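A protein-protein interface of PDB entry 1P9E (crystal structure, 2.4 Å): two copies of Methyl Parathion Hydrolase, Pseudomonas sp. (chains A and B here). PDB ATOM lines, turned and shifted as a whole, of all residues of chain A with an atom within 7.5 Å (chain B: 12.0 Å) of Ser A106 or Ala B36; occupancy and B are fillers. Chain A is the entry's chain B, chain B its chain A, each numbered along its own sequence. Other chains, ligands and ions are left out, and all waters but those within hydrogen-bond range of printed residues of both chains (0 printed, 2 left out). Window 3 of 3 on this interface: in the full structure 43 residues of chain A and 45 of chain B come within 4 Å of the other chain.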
ATOM      1  N   PHE A  55       2.254  -2.763   7.819  1.00  0.00           N
ATOM      2  CA  PHE A  55       3.553  -2.709   7.158  1.00  0.00           C
ATOM      3  C   PHE A  55       3.625  -3.698   6.011  1.00  0.00           C
ATOM      4  O   PHE A  55       2.879  -4.688   5.958  1.00  0.00           O
ATOM      5  CB  PHE A  55       4.688  -2.994   8.141  1.00  0.00           C
ATOM      6  CG  PHE A  55       4.883  -1.925   9.186  1.00  0.00           C
ATOM      7  CD1 PHE A  55       4.122  -0.760   9.168  1.00  0.00           C
ATOM      8  CD2 PHE A  55       5.810  -2.112  10.222  1.00  0.00           C
ATOM      9  CE1 PHE A  55       4.268   0.206  10.161  1.00  0.00           C
ATOM     10  CE2 PHE A  55       5.976  -1.161  11.223  1.00  0.00           C
ATOM     11  CZ  PHE A  55       5.195   0.012  11.196  1.00  0.00           C
ATOM     12  N   ASN A 103       8.410  -1.438   4.420  1.00  0.00           N
ATOM     13  CA  ASN A 103       7.770  -0.166   4.104  1.00  0.00           C
ATOM     14  C   ASN A 103       6.839   0.083   5.267  1.00  0.00           C
ATOM     15  O   ASN A 103       5.884  -0.656   5.461  1.00  0.00           O
ATOM     16  CB  ASN A 103       6.945  -0.239   2.815  1.00  0.00           C
ATOM     17  CG  ASN A 103       6.643   1.137   2.249  1.00  0.00           C
ATOM     18  OD1 ASN A 103       6.439   2.097   2.995  1.00  0.00           O
ATOM     19  ND2 ASN A 103       6.615   1.240   0.925  1.00  0.00           N
ATOM     20  N   THR A 104       7.134   1.115   6.048  1.00  0.00           N
ATOM     21  CA  THR A 104       6.332   1.443   7.218  1.00  0.00           C
ATOM     22  C   THR A 104       5.246   2.449   6.872  1.00  0.00           C
ATOM     23  O   THR A 104       4.493   2.880   7.751  1.00  0.00           O
ATOM     24  CB  THR A 104       7.205   2.071   8.320  1.00  0.00           C
ATOM     25  OG1 THR A 104       7.704   3.341   7.862  1.00  0.00           O
ATOM     26  CG2 THR A 104       8.375   1.145   8.662  1.00  0.00           C
ATOM     27  N   GLY A 105       5.171   2.823   5.602  1.00  0.00           N
ATOM     28  CA  GLY A 105       4.193   3.808   5.202  1.00  0.00           C
ATOM     29  C   GLY A 105       4.895   5.154   5.134  1.00  0.00           C
ATOM     30  O   GLY A 105       4.928   5.794   4.100  1.00  0.00           O
ATOM     31  N   SER A 106       5.485   5.577   6.237  1.00  0.00           N
ATOM     32  CA  SER A 106       6.174   6.847   6.230  1.00  0.00           C
ATOM     33  C   SER A 106       7.662   6.636   5.945  1.00  0.00           C
ATOM     34  O   SER A 106       8.393   7.591   5.665  1.00  0.00           O
ATOM     35  CB  SER A 106       6.019   7.531   7.588  1.00  0.00           C
ATOM     36  OG  SER A 106       6.894   6.939   8.531  1.00  0.00           O
ATOM     37  N   LYS A 107       8.110   5.388   6.032  1.00  0.00           N
ATOM     38  CA  LYS A 107       9.511   5.070   5.808  1.00  0.00           C
ATOM     39  C   LYS A 107       9.736   3.772   5.039  1.00  0.00           C
ATOM     40  O   LYS A 107       8.957   2.820   5.163  1.00  0.00           O
ATOM     41  CB  LYS A 107      10.220   4.980   7.155  1.00  0.00           C
ATOM     42  CG  LYS A 107      10.493   6.317   7.785  1.00  0.00           C
ATOM     43  CD  LYS A 107      11.573   7.022   6.978  1.00  0.00           C
ATOM     44  CE  LYS A 107      11.830   8.420   7.486  1.00  0.00           C
ATOM     45  NZ  LYS A 107      10.653   9.291   7.218  1.00  0.00           N
ATOM     46  N   LEU A 108      10.804   3.746   4.244  1.00  0.00           N
ATOM     47  CA  LEU A 108      11.180   2.552   3.488  1.00  0.00           C
ATOM     48  C   LEU A 108      12.588   2.225   3.972  1.00  0.00           C
ATOM     49  O   LEU A 108      13.515   2.979   3.718  1.00  0.00           O
ATOM     50  CB  LEU A 108      11.206   2.822   1.977  1.00  0.00           C
ATOM     51  CG  LEU A 108      11.584   1.604   1.114  1.00  0.00           C
ATOM     52  CD1 LEU A 108      10.497   0.547   1.200  1.00  0.00           C
ATOM     53  CD2 LEU A 108      11.760   2.020  -0.326  1.00  0.00           C
ATOM     54  N   VAL A 109      12.749   1.119   4.689  1.00  0.00           N
ATOM     55  CA  VAL A 109      14.074   0.768   5.197  1.00  0.00           C
ATOM     56  C   VAL A 109      14.519  -0.603   4.705  1.00  0.00           C
ATOM     57  O   VAL A 109      13.702  -1.497   4.480  1.00  0.00           O
ATOM     58  CB  VAL A 109      14.104   0.792   6.752  1.00  0.00           C
ATOM     59  CG1 VAL A 109      13.623   2.157   7.263  1.00  0.00           C
ATOM     60  CG2 VAL A 109      13.218  -0.293   7.307  1.00  0.00           C
ATOM     61  N   TYR A 135      10.352  -1.183  -6.428  1.00  0.00           N
ATOM     62  CA  TYR A 135      10.906  -0.051  -5.698  1.00  0.00           C
ATOM     63  C   TYR A 135      12.186   0.366  -6.407  1.00  0.00           C
ATOM     64  O   TYR A 135      12.722  -0.381  -7.229  1.00  0.00           O
ATOM     65  CB  TYR A 135      11.223  -0.442  -4.254  1.00  0.00           C
ATOM     66  CG  TYR A 135      10.014  -0.623  -3.372  1.00  0.00           C
ATOM     67  CD1 TYR A 135       9.240   0.472  -3.001  1.00  0.00           C
ATOM     68  CD2 TYR A 135       9.642  -1.892  -2.899  1.00  0.00           C
ATOM     69  CE1 TYR A 135       8.119   0.328  -2.179  1.00  0.00           C
ATOM     70  CE2 TYR A 135       8.514  -2.058  -2.067  1.00  0.00           C
ATOM     71  CZ  TYR A 135       7.758  -0.931  -1.714  1.00  0.00           C
ATOM     72  OH  TYR A 135       6.646  -1.036  -0.904  1.00  0.00           O
ATOM     73  N   GLN A 136      12.664   1.563  -6.095  1.00  0.00           N
ATOM     74  CA  GLN A 136      13.892   2.075  -6.688  1.00  0.00           C
ATOM     75  C   GLN A 136      14.870   2.330  -5.542  1.00  0.00           C
ATOM     76  O   GLN A 136      14.482   2.847  -4.504  1.00  0.00           O
ATOM     77  CB  GLN A 136      13.612   3.397  -7.418  1.00  0.00           C
ATOM     78  CG  GLN A 136      13.617   3.329  -8.949  1.00  0.00           C
ATOM     79  CD  GLN A 136      13.782   4.730  -9.569  1.00  0.00           C
ATOM     80  OE1 GLN A 136      12.940   5.622  -9.353  1.00  0.00           O
ATOM     81  NE2 GLN A 136      14.880   4.933 -10.325  1.00  0.00           N
ATOM     82  N   GLU A 138      16.886   4.581  -4.863  1.00  0.00           N
ATOM     83  CA  GLU A 138      16.834   5.956  -4.385  1.00  0.00           C
ATOM     84  C   GLU A 138      15.684   6.239  -3.446  1.00  0.00           C
ATOM     85  O   GLU A 138      15.645   7.310  -2.849  1.00  0.00           O
ATOM     86  CB  GLU A 138      16.773   6.928  -5.565  1.00  0.00           C
ATOM     87  CG  GLU A 138      17.965   6.806  -6.485  1.00  0.00           C
ATOM     88  CD  GLU A 138      17.692   5.917  -7.679  1.00  0.00           C
ATOM     89  OE1 GLU A 138      16.940   4.913  -7.557  1.00  0.00           O
ATOM     90  OE2 GLU A 138      18.246   6.224  -8.757  1.00  0.00           O
ATOM     91  N   GLN A 139      14.748   5.300  -3.306  1.00  0.00           N
ATOM     92  CA  GLN A 139      13.617   5.515  -2.403  1.00  0.00           C
ATOM     93  C   GLN A 139      13.864   5.004  -0.998  1.00  0.00           C
ATOM     94  O   GLN A 139      13.091   5.311  -0.092  1.00  0.00           O
ATOM     95  CB  GLN A 139      12.341   4.861  -2.930  1.00  0.00           C
ATOM     96  CG  GLN A 139      11.794   5.471  -4.185  1.00  0.00           C
ATOM     97  CD  GLN A 139      10.722   4.607  -4.790  1.00  0.00           C
ATOM     98  OE1 GLN A 139      10.834   3.369  -4.812  1.00  0.00           O
ATOM     99  NE2 GLN A 139       9.674   5.242  -5.298  1.00  0.00           N
ATOM    100  N   VAL A 140      14.921   4.219  -0.815  1.00  0.00           N
ATOM    101  CA  VAL A 140      15.235   3.695   0.505  1.00  0.00           C
ATOM    102  C   VAL A 140      15.708   4.822   1.429  1.00  0.00           C
ATOM    103  O   VAL A 140      16.670   5.549   1.114  1.00  0.00           O
ATOM    104  CB  VAL A 140      16.341   2.610   0.441  1.00  0.00           C
ATOM    105  CG1 VAL A 140      16.684   2.120   1.856  1.00  0.00           C
ATOM    106  CG2 VAL A 140      15.877   1.443  -0.425  1.00  0.00           C
ATOM    107  N   ASP A 141      15.042   4.945   2.578  1.00  0.00           N
ATOM    108  CA  ASP A 141      15.377   5.967   3.559  1.00  0.00           C
ATOM    109  C   ASP A 141      16.481   5.560   4.521  1.00  0.00           C
ATOM    110  O   ASP A 141      17.384   6.343   4.799  1.00  0.00           O
ATOM    111  CB  ASP A 141      14.135   6.353   4.347  1.00  0.00           C
ATOM    112  CG  ASP A 141      13.062   6.944   3.461  1.00  0.00           C
ATOM    113  OD1 ASP A 141      13.453   7.738   2.571  1.00  0.00           O
ATOM    114  OD2 ASP A 141      11.856   6.624   3.649  1.00  0.00           O
ATOM    115  N   GLU A 142      16.410   4.348   5.052  1.00  0.00           N
ATOM    116  CA  GLU A 142      17.441   3.900   5.979  1.00  0.00           C
ATOM    117  C   GLU A 142      17.809   2.454   5.726  1.00  0.00           C
ATOM    118  O   GLU A 142      17.005   1.694   5.181  1.00  0.00           O
ATOM    119  CB  GLU A 142      16.969   4.095   7.416  1.00  0.00           C
ATOM    120  CG  GLU A 142      16.787   5.562   7.736  1.00  0.00           C
ATOM    121  CD  GLU A 142      16.275   5.817   9.133  1.00  0.00           C
ATOM    122  OE1 GLU A 142      16.579   5.018  10.053  1.00  0.00           O
ATOM    123  OE2 GLU A 142      15.573   6.832   9.311  1.00  0.00           O
ATOM    124  N   ASN A 166      20.139   8.132  -1.195  1.00  0.00           N
ATOM    125  CA  ASN A 166      19.331   8.945  -0.288  1.00  0.00           C
ATOM    126  C   ASN A 166      19.148   8.320   1.097  1.00  0.00           C
ATOM    127  O   ASN A 166      18.375   8.826   1.918  1.00  0.00           O
ATOM    128  CB  ASN A 166      17.972   9.216  -0.939  1.00  0.00           C
ATOM    129  CG  ASN A 166      18.099  10.038  -2.208  1.00  0.00           C
ATOM    130  OD1 ASN A 166      17.696   9.609  -3.298  1.00  0.00           O
ATOM    131  ND2 ASN A 166      18.685  11.232  -2.076  1.00  0.00           N
ATOM    132  N   VAL A 223      13.235   4.122  13.291  1.00  0.00           N
ATOM    133  CA  VAL A 223      11.970   4.695  12.876  1.00  0.00           C
ATOM    134  C   VAL A 223      10.833   3.969  13.603  1.00  0.00           C
ATOM    135  O   VAL A 223      11.003   2.827  14.060  1.00  0.00           O
ATOM    136  CB  VAL A 223      11.750   4.525  11.387  1.00  0.00           C
ATOM    137  CG1 VAL A 223      12.837   5.249  10.627  1.00  0.00           C
ATOM    138  CG2 VAL A 223      11.714   3.029  11.044  1.00  0.00           C
ATOM    139  N   PRO A 224       9.662   4.623  13.738  1.00  0.00           N
ATOM    140  CA  PRO A 224       8.509   4.007  14.412  1.00  0.00           C
ATOM    141  C   PRO A 224       8.228   2.633  13.798  1.00  0.00           C
ATOM    142  O   PRO A 224       8.213   2.494  12.576  1.00  0.00           O
ATOM    143  CB  PRO A 224       7.376   4.997  14.135  1.00  0.00           C
ATOM    144  CG  PRO A 224       8.111   6.331  14.148  1.00  0.00           C
ATOM    145  CD  PRO A 224       9.390   6.026  13.376  1.00  0.00           C
ATOM    146  N   ALA B  36      11.155   7.549   1.021  1.00  0.00           N
ATOM    147  CA  ALA B  36       9.892   6.771   1.218  1.00  0.00           C
ATOM    148  C   ALA B  36       9.327   6.334  -0.124  1.00  0.00           C
ATOM    149  O   ALA B  36       9.775   6.771  -1.188  1.00  0.00           O
ATOM    150  CB  ALA B  36       8.846   7.610   1.965  1.00  0.00           C
ATOM    151  N   ALA B  37       8.331   5.461  -0.069  1.00  0.00           N
ATOM    152  CA  ALA B  37       7.710   4.987  -1.282  1.00  0.00           C
ATOM    153  C   ALA B  37       6.336   4.453  -0.941  1.00  0.00           C
ATOM    154  O   ALA B  37       6.096   4.047   0.184  1.00  0.00           O
ATOM    155  CB  ALA B  37       8.564   3.895  -1.903  1.00  0.00           C
ATOM    156  N   PRO B  38       5.406   4.475  -1.906  1.00  0.00           N
ATOM    157  CA  PRO B  38       4.061   3.961  -1.632  1.00  0.00           C
ATOM    158  C   PRO B  38       4.149   2.438  -1.636  1.00  0.00           C
ATOM    159  O   PRO B  38       4.942   1.878  -2.393  1.00  0.00           O
ATOM    160  CB  PRO B  38       3.239   4.511  -2.796  1.00  0.00           C
ATOM    161  CG  PRO B  38       4.237   4.548  -3.926  1.00  0.00           C
ATOM    162  CD  PRO B  38       5.497   5.065  -3.253  1.00  0.00           C
ATOM    163  N   GLN B  39       3.370   1.770  -0.784  1.00  0.00           N
ATOM    164  CA  GLN B  39       3.408   0.304  -0.720  1.00  0.00           C
ATOM    165  C   GLN B  39       2.890  -0.236  -2.044  1.00  0.00           C
ATOM    166  O   GLN B  39       1.850   0.215  -2.561  1.00  0.00           O
ATOM    167  CB  GLN B  39       2.544  -0.247   0.436  1.00  0.00           C
ATOM    168  CG  GLN B  39       2.846   0.332   1.812  1.00  0.00           C
ATOM    169  CD  GLN B  39       2.371  -0.559   2.970  1.00  0.00           C
ATOM    170  OE1 GLN B  39       1.434  -1.362   2.767  1.00  0.00           O
ATOM    171  NE2 GLN B  39       2.921  -0.439   4.100  1.00  0.00           N
ATOM    172  N   VAL B  40       3.619  -1.208  -2.593  1.00  0.00           N
ATOM    173  CA  VAL B  40       3.240  -1.805  -3.865  1.00  0.00           C
ATOM    174  C   VAL B  40       2.127  -2.829  -3.649  1.00  0.00           C
ATOM    175  O   VAL B  40       1.185  -2.926  -4.443  1.00  0.00           O
ATOM    176  CB  VAL B  40       4.472  -2.465  -4.546  1.00  0.00           C
ATOM    177  CG1 VAL B  40       4.108  -2.971  -5.919  1.00  0.00           C
ATOM    178  CG2 VAL B  40       5.602  -1.444  -4.662  1.00  0.00           C
ATOM    179  N   ARG B  41       2.230  -3.563  -2.548  1.00  0.00           N
ATOM    180  CA  ARG B  41       1.265  -4.594  -2.180  1.00  0.00           C
ATOM    181  C   ARG B  41       0.831  -5.563  -3.292  1.00  0.00           C
ATOM    182  O   ARG B  41      -0.371  -5.740  -3.546  1.00  0.00           O
ATOM    183  CB  ARG B  41       0.010  -3.975  -1.550  1.00  0.00           C
ATOM    184  CG  ARG B  41       0.206  -3.278  -0.209  1.00  0.00           C
ATOM    185  CD  ARG B  41      -1.130  -3.206   0.523  1.00  0.00           C
ATOM    186  NE  ARG B  41      -1.262  -2.062   1.433  1.00  0.00           N
ATOM    187  CZ  ARG B  41      -1.800  -0.881   1.105  1.00  0.00           C
ATOM    188  NH1 ARG B  41      -2.266  -0.662  -0.122  1.00  0.00           N
ATOM    189  NH2 ARG B  41      -1.896   0.083   2.018  1.00  0.00           N
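Of the 6 printed residues of chain B, 5 touch a printed residue of chain A.
Printed residues of chain A that touch a printed residue of chain B: Phe A55, Asn A103, Ser A106, Tyr A135, Gln A139 and Asp A141.
Among the printed residues, no Asp or Glu carboxylate lies within 4 Å of a Lys or Arg side-chain nitrogen of the other chain.
Among the printed residues, merely in contact across the chains: Phe A55 with Gln B39, Asn A103 with Pro B38, Ser A106 with Ala B36, Tyr A135 with Ala B37, Tyr A135 with Pro B38, Tyr A135 with Gln B39 and Gln A139 with Ala B37.
Asn A103 touches just these residues of chain B: Ala B37, Pro B38 and Gln B39.
No residue of chain B comes within 4 Å of Thr A104.
No residue of chain B comes within 4 Å of Gly A105.
No residue of chain B comes within 4 Å of Lys A107.
No residue of chain B comes within 4 Å of Leu A108.
Asp A141 touches one residue of chain B.
Val A223 touches none of the printed residues of chain B.
No residue of chain B comes within 4 Å of Pro A224.
Of the printed residues of chain A, Ala B37 touches Asn A103, Tyr A135 and Gln A139.
Of the printed residues of chain A, Gln B39 touches Phe A55 (3.8 Å), Asn A103 (3.3 Å) and Tyr A135 (3.5 Å).
The nearest residue of chain B that does not touch Ser A106 is Ala B37 (6.1 Å).
The nearest printed residue of chain A that does not touch Ala B37 is Leu A108 (4.03 Å).
OD1 of Asn A103 lies within hydrogen-bond range of N of Gly A105, at 3.0 Å.
The side-chain amide nitrogen (ND2) of Asn A103 sits at hydrogen-bond distance from the side-chain hydroxyl (OH) of Tyr A135, 2.9 Å away.
The backbone NH of Gln A136 lies within hydrogen-bond range of the side-chain amide oxygen of Gln A139.
O of Lys A107 sits close to OD1 of Asn A103.
The backbone carbonyl oxygen (O) of Leu A108 sits at hydrogen-bond distance from the backbone NH (N) of Asp A141 (2.7 Å).
The side-chain amide oxygen (OE1) of Gln B39 is in hydrogen-bond range of the guanidinium group (NE) of Arg B41, at 3.1 Å.
No position is printed for both chains.
The backbone NH (N) of Ala B36 lies within hydrogen-bond range of the backbone carbonyl oxygen (O) of Gln A139.
The side-chain amide nitrogen (ND2) of Asn A103 is in hydrogen-bond range of the backbone carbonyl oxygen (O) of Ala B37 (2.9 Å).
The backbone carbonyl oxygen (O) of Asn A103 is in hydrogen-bond range of the side-chain amide nitrogen (NE2) of Gln B39 (3.3 Å).
The backbone NH (N) of Val B40 is in hydrogen-bond range of the side-chain hydroxyl (OH) of Tyr A135, at 3.5 Å.
N of Ala B36 lies within hydrogen-bond range of OD1 of Asp A141, at 2.8 Å.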
